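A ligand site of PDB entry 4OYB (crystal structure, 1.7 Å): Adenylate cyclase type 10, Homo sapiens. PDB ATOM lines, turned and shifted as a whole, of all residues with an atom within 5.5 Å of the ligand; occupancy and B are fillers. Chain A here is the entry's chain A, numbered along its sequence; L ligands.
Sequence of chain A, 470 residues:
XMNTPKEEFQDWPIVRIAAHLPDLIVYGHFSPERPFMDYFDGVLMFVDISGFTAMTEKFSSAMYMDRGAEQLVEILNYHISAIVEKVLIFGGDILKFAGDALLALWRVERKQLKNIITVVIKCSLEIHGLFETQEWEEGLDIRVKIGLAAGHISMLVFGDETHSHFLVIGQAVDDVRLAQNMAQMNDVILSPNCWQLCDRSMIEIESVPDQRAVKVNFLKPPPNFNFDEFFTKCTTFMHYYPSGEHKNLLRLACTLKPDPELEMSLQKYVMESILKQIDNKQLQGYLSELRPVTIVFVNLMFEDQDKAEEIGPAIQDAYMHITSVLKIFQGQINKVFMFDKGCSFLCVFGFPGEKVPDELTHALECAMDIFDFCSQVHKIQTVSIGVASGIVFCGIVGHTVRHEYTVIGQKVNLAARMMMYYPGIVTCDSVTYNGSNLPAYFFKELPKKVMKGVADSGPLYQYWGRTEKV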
ATOM      1  N   PHE A  46      -9.640  11.922  33.202  1.00  0.00           N
ATOM      2  CA  PHE A  46      -8.886  11.062  32.297  1.00  0.00           C
ATOM      3  C   PHE A  46      -7.476  11.577  32.296  1.00  0.00           C
ATOM      4  O   PHE A  46      -7.234  12.718  31.910  1.00  0.00           O
ATOM      5  CB  PHE A  46      -9.524  11.121  30.918  1.00  0.00           C
ATOM      6  CG  PHE A  46      -9.179   9.979  29.996  1.00  0.00           C
ATOM      7  CD1 PHE A  46      -9.085   8.672  30.464  1.00  0.00           C
ATOM      8  CD2 PHE A  46      -8.943  10.214  28.664  1.00  0.00           C
ATOM      9  CE1 PHE A  46      -8.763   7.634  29.620  1.00  0.00           C
ATOM     10  CE2 PHE A  46      -8.624   9.175  27.806  1.00  0.00           C
ATOM     11  CZ  PHE A  46      -8.532   7.882  28.287  1.00  0.00           C
ATOM     12  N   LEU A  95     -11.604   3.760  37.696  1.00  0.00           N
ATOM     13  CA  LEU A  95     -12.440   2.798  36.918  1.00  0.00           C
ATOM     14  C   LEU A  95     -11.644   1.740  36.147  1.00  0.00           C
ATOM     15  O   LEU A  95     -11.919   0.543  36.284  1.00  0.00           O
ATOM     16  CB  LEU A  95     -13.391   3.533  35.977  1.00  0.00           C
ATOM     17  CG  LEU A  95     -14.411   4.468  36.605  1.00  0.00           C
ATOM     18  CD1 LEU A  95     -15.364   4.999  35.540  1.00  0.00           C
ATOM     19  CD2 LEU A  95     -15.138   3.778  37.738  1.00  0.00           C
ATOM     20  N   LYS A  96     -10.665   2.167  35.335  1.00  0.00           N
ATOM     21  CA  LYS A  96      -9.789   1.261  34.553  1.00  0.00           C
ATOM     22  C   LYS A  96      -8.477   1.909  34.246  1.00  0.00           C
ATOM     23  O   LYS A  96      -8.367   3.146  34.226  1.00  0.00           O
ATOM     24  CB  LYS A  96     -10.391   0.887  33.157  1.00  0.00           C
ATOM     25  CG  LYS A  96     -11.619   0.047  33.200  1.00  0.00           C
ATOM     26  CD  LYS A  96     -12.005  -0.448  31.820  1.00  0.00           C
ATOM     27  CE  LYS A  96     -13.423  -0.944  31.872  1.00  0.00           C
ATOM     28  NZ  LYS A  96     -13.770  -1.899  30.787  1.00  0.00           N
ATOM     29  N   PHE A  97      -7.490   1.055  34.003  1.00  0.00           N
ATOM     30  CA  PHE A  97      -6.172   1.427  33.531  1.00  0.00           C
ATOM     31  C   PHE A  97      -6.033   0.911  32.105  1.00  0.00           C
ATOM     32  O   PHE A  97      -6.526  -0.166  31.772  1.00  0.00           O
ATOM     33  CB  PHE A  97      -5.050   0.791  34.330  1.00  0.00           C
ATOM     34  CG  PHE A  97      -4.978   1.147  35.781  1.00  0.00           C
ATOM     35  CD1 PHE A  97      -5.756   0.470  36.707  1.00  0.00           C
ATOM     36  CD2 PHE A  97      -4.132   2.155  36.244  1.00  0.00           C
ATOM     37  CE1 PHE A  97      -5.717   0.769  38.053  1.00  0.00           C
ATOM     38  CE2 PHE A  97      -4.089   2.470  37.588  1.00  0.00           C
ATOM     39  CZ  PHE A  97      -4.872   1.769  38.495  1.00  0.00           C
ATOM     40  N   ALA A  98      -5.339   1.689  31.277  1.00  0.00           N
ATOM     41  CA  ALA A  98      -4.835   1.238  29.977  1.00  0.00           C
ATOM     42  C   ALA A  98      -3.396   1.737  29.827  1.00  0.00           C
ATOM     43  O   ALA A  98      -2.971   2.629  30.561  1.00  0.00           O
ATOM     44  CB  ALA A  98      -5.666   1.819  28.856  1.00  0.00           C
ATOM     45  N   ALA A 101      -3.613   5.570  29.451  1.00  0.00           N
ATOM     46  CA  ALA A 101      -4.407   6.330  30.391  1.00  0.00           C
ATOM     47  C   ALA A 101      -4.956   5.602  31.664  1.00  0.00           C
ATOM     48  O   ALA A 101      -4.911   4.379  31.811  1.00  0.00           O
ATOM     49  CB  ALA A 101      -5.556   6.970  29.625  1.00  0.00           C
ATOM     50  N   LEU A 102      -5.475   6.386  32.599  1.00  0.00           N
ATOM     51  CA  LEU A 102      -6.414   5.836  33.571  1.00  0.00           C
ATOM     52  C   LEU A 102      -7.602   6.797  33.645  1.00  0.00           C
ATOM     53  O   LEU A 102      -7.462   8.003  33.405  1.00  0.00           O
ATOM     54  CB  LEU A 102      -5.793   5.595  34.943  1.00  0.00           C
ATOM     55  CG  LEU A 102      -5.248   6.792  35.721  1.00  0.00           C
ATOM     56  CD1 LEU A 102      -6.333   7.440  36.538  1.00  0.00           C
ATOM     57  CD2 LEU A 102      -4.138   6.294  36.666  1.00  0.00           C
ATOM     58  N   LEU A 103      -8.760   6.239  33.960  1.00  0.00           N
ATOM     59  CA  LEU A 103     -10.011   6.955  34.054  1.00  0.00           C
ATOM     60  C   LEU A 103     -10.522   6.854  35.476  1.00  0.00           C
ATOM     61  O   LEU A 103     -10.626   5.749  36.006  1.00  0.00           O
ATOM     62  CB  LEU A 103     -11.026   6.298  33.112  1.00  0.00           C
ATOM     63  CG  LEU A 103     -12.456   6.861  33.115  1.00  0.00           C
ATOM     64  CD1 LEU A 103     -12.432   8.299  32.623  1.00  0.00           C
ATOM     65  CD2 LEU A 103     -13.383   6.002  32.261  1.00  0.00           C
ATOM     66  N   PHE A 166     -17.491  -4.272  32.401  1.00  0.00           N
ATOM     67  CA  PHE A 166     -18.249  -3.036  32.474  1.00  0.00           C
ATOM     68  C   PHE A 166     -17.613  -1.915  31.650  1.00  0.00           C
ATOM     69  O   PHE A 166     -16.401  -1.921  31.309  1.00  0.00           O
ATOM     70  CB  PHE A 166     -18.427  -2.543  33.930  1.00  0.00           C
ATOM     71  CG  PHE A 166     -17.222  -1.805  34.440  1.00  0.00           C
ATOM     72  CD1 PHE A 166     -17.162  -0.413  34.370  1.00  0.00           C
ATOM     73  CD2 PHE A 166     -16.168  -2.486  35.003  1.00  0.00           C
ATOM     74  CE1 PHE A 166     -16.061   0.255  34.833  1.00  0.00           C
ATOM     75  CE2 PHE A 166     -15.041  -1.793  35.473  1.00  0.00           C
ATOM     76  CZ  PHE A 166     -15.013  -0.444  35.384  1.00  0.00           C
ATOM     77  N   LEU A 167     -18.477  -0.958  31.343  1.00  0.00           N
ATOM     78  CA  LEU A 167     -18.138   0.316  30.741  1.00  0.00           C
ATOM     79  C   LEU A 167     -18.970   1.432  31.306  1.00  0.00           C
ATOM     80  O   LEU A 167     -20.135   1.227  31.679  1.00  0.00           O
ATOM     81  CB  LEU A 167     -18.420   0.297  29.245  1.00  0.00           C
ATOM     82  CG  LEU A 167     -17.594  -0.605  28.394  1.00  0.00           C
ATOM     83  CD1 LEU A 167     -18.268  -0.780  27.029  1.00  0.00           C
ATOM     84  CD2 LEU A 167     -16.228   0.039  28.271  1.00  0.00           C
ATOM     85  N   VAL A 168     -18.391   2.622  31.384  1.00  0.00           N
ATOM     86  CA  VAL A 168     -19.197   3.809  31.455  1.00  0.00           C
ATOM     87  C   VAL A 168     -19.267   4.433  30.079  1.00  0.00           C
ATOM     88  O   VAL A 168     -18.274   4.425  29.291  1.00  0.00           O
ATOM     89  CB  VAL A 168     -18.719   4.839  32.517  1.00  0.00           C
ATOM     90  CG1 VAL A 168     -18.971   4.309  33.900  1.00  0.00           C
ATOM     91  CG2 VAL A 168     -17.282   5.268  32.335  1.00  0.00           C
ATOM     92  N   ILE A 169     -20.432   4.984  29.770  1.00  0.00           N
ATOM     93  CA  ILE A 169     -20.664   5.612  28.463  1.00  0.00           C
ATOM     94  C   ILE A 169     -21.487   6.875  28.540  1.00  0.00           C
ATOM     95  O   ILE A 169     -21.997   7.229  29.594  1.00  0.00           O
ATOM     96  CB  ILE A 169     -21.330   4.613  27.494  1.00  0.00           C
ATOM     97  CG1 ILE A 169     -22.776   4.382  27.889  1.00  0.00           C
ATOM     98  CG2 ILE A 169     -20.556   3.284  27.474  1.00  0.00           C
ATOM     99  CD1 ILE A 169     -23.576   3.628  26.852  1.00  0.00           C
ATOM    100  N   VAL A 173     -18.646  10.904  29.221  1.00  0.00           N
ATOM    101  CA  VAL A 173     -17.550  10.009  28.908  1.00  0.00           C
ATOM    102  C   VAL A 173     -16.833  10.432  27.599  1.00  0.00           C
ATOM    103  O   VAL A 173     -15.628  10.526  27.556  1.00  0.00           O
ATOM    104  CB  VAL A 173     -18.034   8.544  28.864  1.00  0.00           C
ATOM    105  CG1 VAL A 173     -16.920   7.651  28.381  1.00  0.00           C
ATOM    106  CG2 VAL A 173     -18.529   8.131  30.245  1.00  0.00           C
ATOM    107  N   ARG A 177     -12.670  12.316  27.104  1.00  0.00           N
ATOM    108  CA  ARG A 177     -11.669  11.918  26.108  1.00  0.00           C
ATOM    109  C   ARG A 177     -11.292  13.113  25.236  1.00  0.00           C
ATOM    110  O   ARG A 177     -10.107  13.391  25.035  1.00  0.00           O
ATOM    111  CB  ARG A 177     -12.181  10.774  25.226  1.00  0.00           C
ATOM    112  CG  ARG A 177     -11.187  10.276  24.172  1.00  0.00           C
ATOM    113  CD  ARG A 177     -10.191   9.261  24.717  1.00  0.00           C
ATOM    114  NE  ARG A 177      -8.816   9.556  24.318  1.00  0.00           N
ATOM    115  CZ  ARG A 177      -7.795   8.716  24.449  1.00  0.00           C
ATOM    116  NH1 ARG A 177      -7.986   7.516  24.959  1.00  0.00           N
ATOM    117  NH2 ARG A 177      -6.576   9.078  24.056  1.00  0.00           N
ATOM    118  N   PHE A 297      -7.683  -5.921  17.786  1.00  0.00           N
ATOM    119  CA  PHE A 297      -8.352  -4.787  18.375  1.00  0.00           C
ATOM    120  C   PHE A 297      -9.633  -4.563  17.560  1.00  0.00           C
ATOM    121  O   PHE A 297      -9.580  -4.167  16.377  1.00  0.00           O
ATOM    122  CB  PHE A 297      -7.448  -3.559  18.401  1.00  0.00           C
ATOM    123  CG  PHE A 297      -7.516  -2.747  19.685  1.00  0.00           C
ATOM    124  CD1 PHE A 297      -8.708  -2.496  20.354  1.00  0.00           C
ATOM    125  CD2 PHE A 297      -6.339  -2.233  20.215  1.00  0.00           C
ATOM    126  CE1 PHE A 297      -8.711  -1.740  21.535  1.00  0.00           C
ATOM    127  CE2 PHE A 297      -6.333  -1.488  21.366  1.00  0.00           C
ATOM    128  CZ  PHE A 297      -7.524  -1.244  22.027  1.00  0.00           C
ATOM    129  N   VAL A 336     -11.949  -3.658  27.604  1.00  0.00           N
ATOM    130  CA  VAL A 336     -12.977  -3.084  26.768  1.00  0.00           C
ATOM    131  C   VAL A 336     -13.062  -1.602  27.097  1.00  0.00           C
ATOM    132  O   VAL A 336     -13.037  -1.201  28.265  1.00  0.00           O
ATOM    133  CB  VAL A 336     -14.348  -3.783  26.917  1.00  0.00           C
ATOM    134  CG1 VAL A 336     -15.298  -3.288  25.846  1.00  0.00           C
ATOM    135  CG2 VAL A 336     -14.235  -5.302  26.845  1.00  0.00           C
ATOM    136  N   PHE A 337     -13.144  -0.783  26.065  1.00  0.00           N
ATOM    137  CA  PHE A 337     -13.065   0.652  26.155  1.00  0.00           C
ATOM    138  C   PHE A 337     -14.168   1.235  25.297  1.00  0.00           C
ATOM    139  O   PHE A 337     -14.600   0.640  24.322  1.00  0.00           O
ATOM    140  CB  PHE A 337     -11.744   1.186  25.593  1.00  0.00           C
ATOM    141  CG  PHE A 337     -10.511   0.650  26.227  1.00  0.00           C
ATOM    142  CD1 PHE A 337      -9.474   0.142  25.447  1.00  0.00           C
ATOM    143  CD2 PHE A 337     -10.368   0.647  27.607  1.00  0.00           C
ATOM    144  CE1 PHE A 337      -8.333  -0.369  26.011  1.00  0.00           C
ATOM    145  CE2 PHE A 337      -9.202   0.138  28.188  1.00  0.00           C
ATOM    146  CZ  PHE A 337      -8.191  -0.365  27.398  1.00  0.00           C
ATOM    147  N   MET A 338     -14.629   2.408  25.655  1.00  0.00           N
ATOM    148  CA  MET A 338     -15.610   3.092  24.831  1.00  0.00           C
ATOM    149  C   MET A 338     -15.652   4.576  25.065  1.00  0.00           C
ATOM    150  O   MET A 338     -15.862   5.039  26.175  1.00  0.00           O
ATOM    151  CB  MET A 338     -17.002   2.535  25.091  1.00  0.00           C
ATOM    152  CG  MET A 338     -18.036   3.273  24.275  1.00  0.00           C
ATOM    153  SD  MET A 338     -19.450   2.267  24.026  1.00  0.00           S
ATOM    154  CE  MET A 338     -20.398   3.451  23.107  1.00  0.00           C
ATOM    155  N   PHE A 339     -15.452   5.339  24.010  1.00  0.00           N
ATOM    156  CA  PHE A 339     -15.651   6.786  24.111  1.00  0.00           C
ATOM    157  C   PHE A 339     -16.605   7.219  23.016  1.00  0.00           C
ATOM    158  O   PHE A 339     -17.783   6.818  23.029  1.00  0.00           O
ATOM    159  CB  PHE A 339     -14.303   7.520  24.123  1.00  0.00           C
ATOM    160  CG  PHE A 339     -13.559   7.367  25.415  1.00  0.00           C
ATOM    161  CD1 PHE A 339     -12.430   6.562  25.502  1.00  0.00           C
ATOM    162  CD2 PHE A 339     -13.989   8.039  26.549  1.00  0.00           C
ATOM    163  CE1 PHE A 339     -11.747   6.425  26.697  1.00  0.00           C
ATOM    164  CE2 PHE A 339     -13.304   7.902  27.758  1.00  0.00           C
ATOM    165  CZ  PHE A 339     -12.178   7.097  27.831  1.00  0.00           C
ATOM    166  N   LYS A 341     -15.676   7.116  19.805  1.00  0.00           N
ATOM    167  CA  LYS A 341     -15.184   6.385  18.641  1.00  0.00           C
ATOM    168  C   LYS A 341     -15.777   5.000  18.499  1.00  0.00           C
ATOM    169  O   LYS A 341     -15.461   4.296  17.534  1.00  0.00           O
ATOM    170  CB  LYS A 341     -13.671   6.255  18.747  1.00  0.00           C
ATOM    171  CG  LYS A 341     -13.092   6.850  20.032  1.00  0.00           C
ATOM    172  CD  LYS A 341     -12.909   5.811  21.130  1.00  0.00           C
ATOM    173  CE  LYS A 341     -11.892   4.758  20.720  1.00  0.00           C
ATOM    174  NZ  LYS A 341     -12.558   3.719  19.876  1.00  0.00           N
ATOM    175  N   SER A 344     -14.582  -0.638  21.885  1.00  0.00           N
ATOM    176  CA  SER A 344     -13.420  -1.405  21.399  1.00  0.00           C
ATOM    177  C   SER A 344     -13.006  -2.518  22.369  1.00  0.00           C
ATOM    178  O   SER A 344     -12.945  -2.346  23.588  1.00  0.00           O
ATOM    179  CB  SER A 344     -12.267  -0.498  20.992  1.00  0.00           C
ATOM    180  OG  SER A 344     -11.620   0.073  22.099  1.00  0.00           O
ATOM    181  N   ALA A 416      -4.695  -0.398  17.442  1.00  0.00           N
ATOM    182  CA  ALA A 416      -5.751   0.557  17.801  1.00  0.00           C
ATOM    183  C   ALA A 416      -5.914   1.664  16.768  1.00  0.00           C
ATOM    184  O   ALA A 416      -7.008   2.119  16.508  1.00  0.00           O
ATOM    185  CB  ALA A 416      -5.460   1.197  19.162  1.00  0.00           C
ATOM    186  N   MET A 419      -7.598   0.150  13.419  1.00  0.00           N
ATOM    187  CA  MET A 419      -9.043  -0.014  13.448  1.00  0.00           C
ATOM    188  C   MET A 419      -9.789   1.322  13.209  1.00  0.00           C
ATOM    189  O   MET A 419     -10.882   1.311  12.718  1.00  0.00           O
ATOM    190  CB  MET A 419      -9.518  -0.737  14.713  1.00  0.00           C
ATOM    191  CG  MET A 419      -9.537   0.118  15.949  1.00  0.00           C
ATOM    192  SD  MET A 419      -9.814  -0.834  17.450  1.00  0.00           S
ATOM    193  CE  MET A 419      -9.677   0.555  18.564  1.00  0.00           C
HETATM  194  C1  LIG L   1      -9.249   2.158  22.048  1.00  0.00           C
HETATM  195  C2  LIG L   1      -9.405   3.274  23.086  1.00  0.00           C
HETATM  196  C3  LIG L   1      -7.871   3.262  26.451  1.00  0.00           C
HETATM  197  C4  LIG L   1      -8.760   4.028  28.551  1.00  0.00           C
HETATM  198  C5  LIG L   1      -9.261   3.947  30.894  1.00  0.00           C
HETATM  199  C6  LIG L   1     -10.591   3.734  30.608  1.00  0.00           C
HETATM  200  C7  LIG L   1     -11.024   3.668  29.289  1.00  0.00           C
HETATM  201  C8  LIG L   1     -10.091   3.814  28.265  1.00  0.00           C
HETATM  202  C9  LIG L   1     -12.440   3.445  28.897  1.00  0.00           C
HETATM  203  C10 LIG L   1     -13.489   3.034  29.867  1.00  0.00           C
HETATM  204  O1  LIG L   1      -8.638   2.918  24.270  1.00  0.00           O
HETATM  205  C11 LIG L   1      -8.598   3.823  25.268  1.00  0.00           C
HETATM  206  O2  LIG L   1      -9.073   4.936  25.213  1.00  0.00           O
HETATM  207  O3  LIG L   1      -7.817   4.185  27.546  1.00  0.00           O
HETATM  208  C12 LIG L   1      -8.341   4.096  29.865  1.00  0.00           C
HETATM  209  O4  LIG L   1     -12.757   3.612  27.722  1.00  0.00           O
HETATM  210  N1  LIG L   1     -13.241   2.438  31.004  1.00  0.00           N
HETATM  211  O5  LIG L   1     -14.482   2.238  31.587  1.00  0.00           O
HETATM  212  N2  LIG L   1     -15.487   2.707  30.818  1.00  0.00           N
HETATM  213  C13 LIG L   1     -14.904   3.194  29.762  1.00  0.00           C
HETATM  214  N3  LIG L   1     -15.591   3.776  28.750  1.00  0.00           N
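O2 of the ligand is in hydrogen-bond range of NH1 of Arg 177 (2.8 Å). The backbone NH (N) of Val 168 is in hydrogen-bond range of a nitrogen (N2) of the ligand (3.0 Å). The backbone carbonyl oxygen (O) of Val 168 is in hydrogen-bond range of a nitrogen (N3) of the ligand, 2.8 Å away. O4 of the ligand sits at hydrogen-bond distance from N of Met 338. O of Met 338 is in hydrogen-bond range of N3 of the ligand (2.9 Å).
CE1 of Phe 46 touches C12 of the ligand (3.6 Å). Lys 96 touches the ligand. Ala 98 touches the ligand. Ala 101 touches the ligand. Leu 103 touches the ligand. CA of Leu 167 touches N2 of the ligand (3.6 Å). CZ of Phe 297 touches C1 of the ligand, 3.8 Å away. Phe 337 touches the ligand (CD1 to O1, 3.1 Å). Phe 339 touches the ligand (CE1 to O4, 3.2 Å). Lys 341 touches the ligand. Ser 344 touches the ligand (OG to C1, 3.2 Å). Met 419 touches the ligand. Hydrophobic or aromatic side chains within 4 Å of the ligand: Phe 46, Ala 98, Leu 103, Leu 167, Val 168, Phe 297, Phe 337, Phe 339 and Met 419. Within 4 Å of the ligand: Phe 46, Lys 96, Ala 98, Ala 101, Leu 103, Leu 167, Val 168, Arg 177, Phe 297, Phe 337, Met 338, Phe 339, Lys 341, Ser 344 and Met 419. The nearest printed residue that does not touch the ligand is Val 173 (4.1 Å).
N of Ser 344 sits at hydrogen-bond distance from O of Phe 337, at 2.8 Å. The backbone carbonyl oxygen (O) of Lys 96 is in hydrogen-bond range of the backbone NH (N) of Leu 103, at 3.1 Å. NZ of Lys 96 sits at hydrogen-bond distance from O of Phe 166, at 2.7 Å. The side-chain amino group of Lys 96 is in hydrogen-bond range of the backbone carbonyl oxygen of Val 336, at 2.7 Å. N of Leu 95 sits at hydrogen-bond distance from O of Leu 103.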
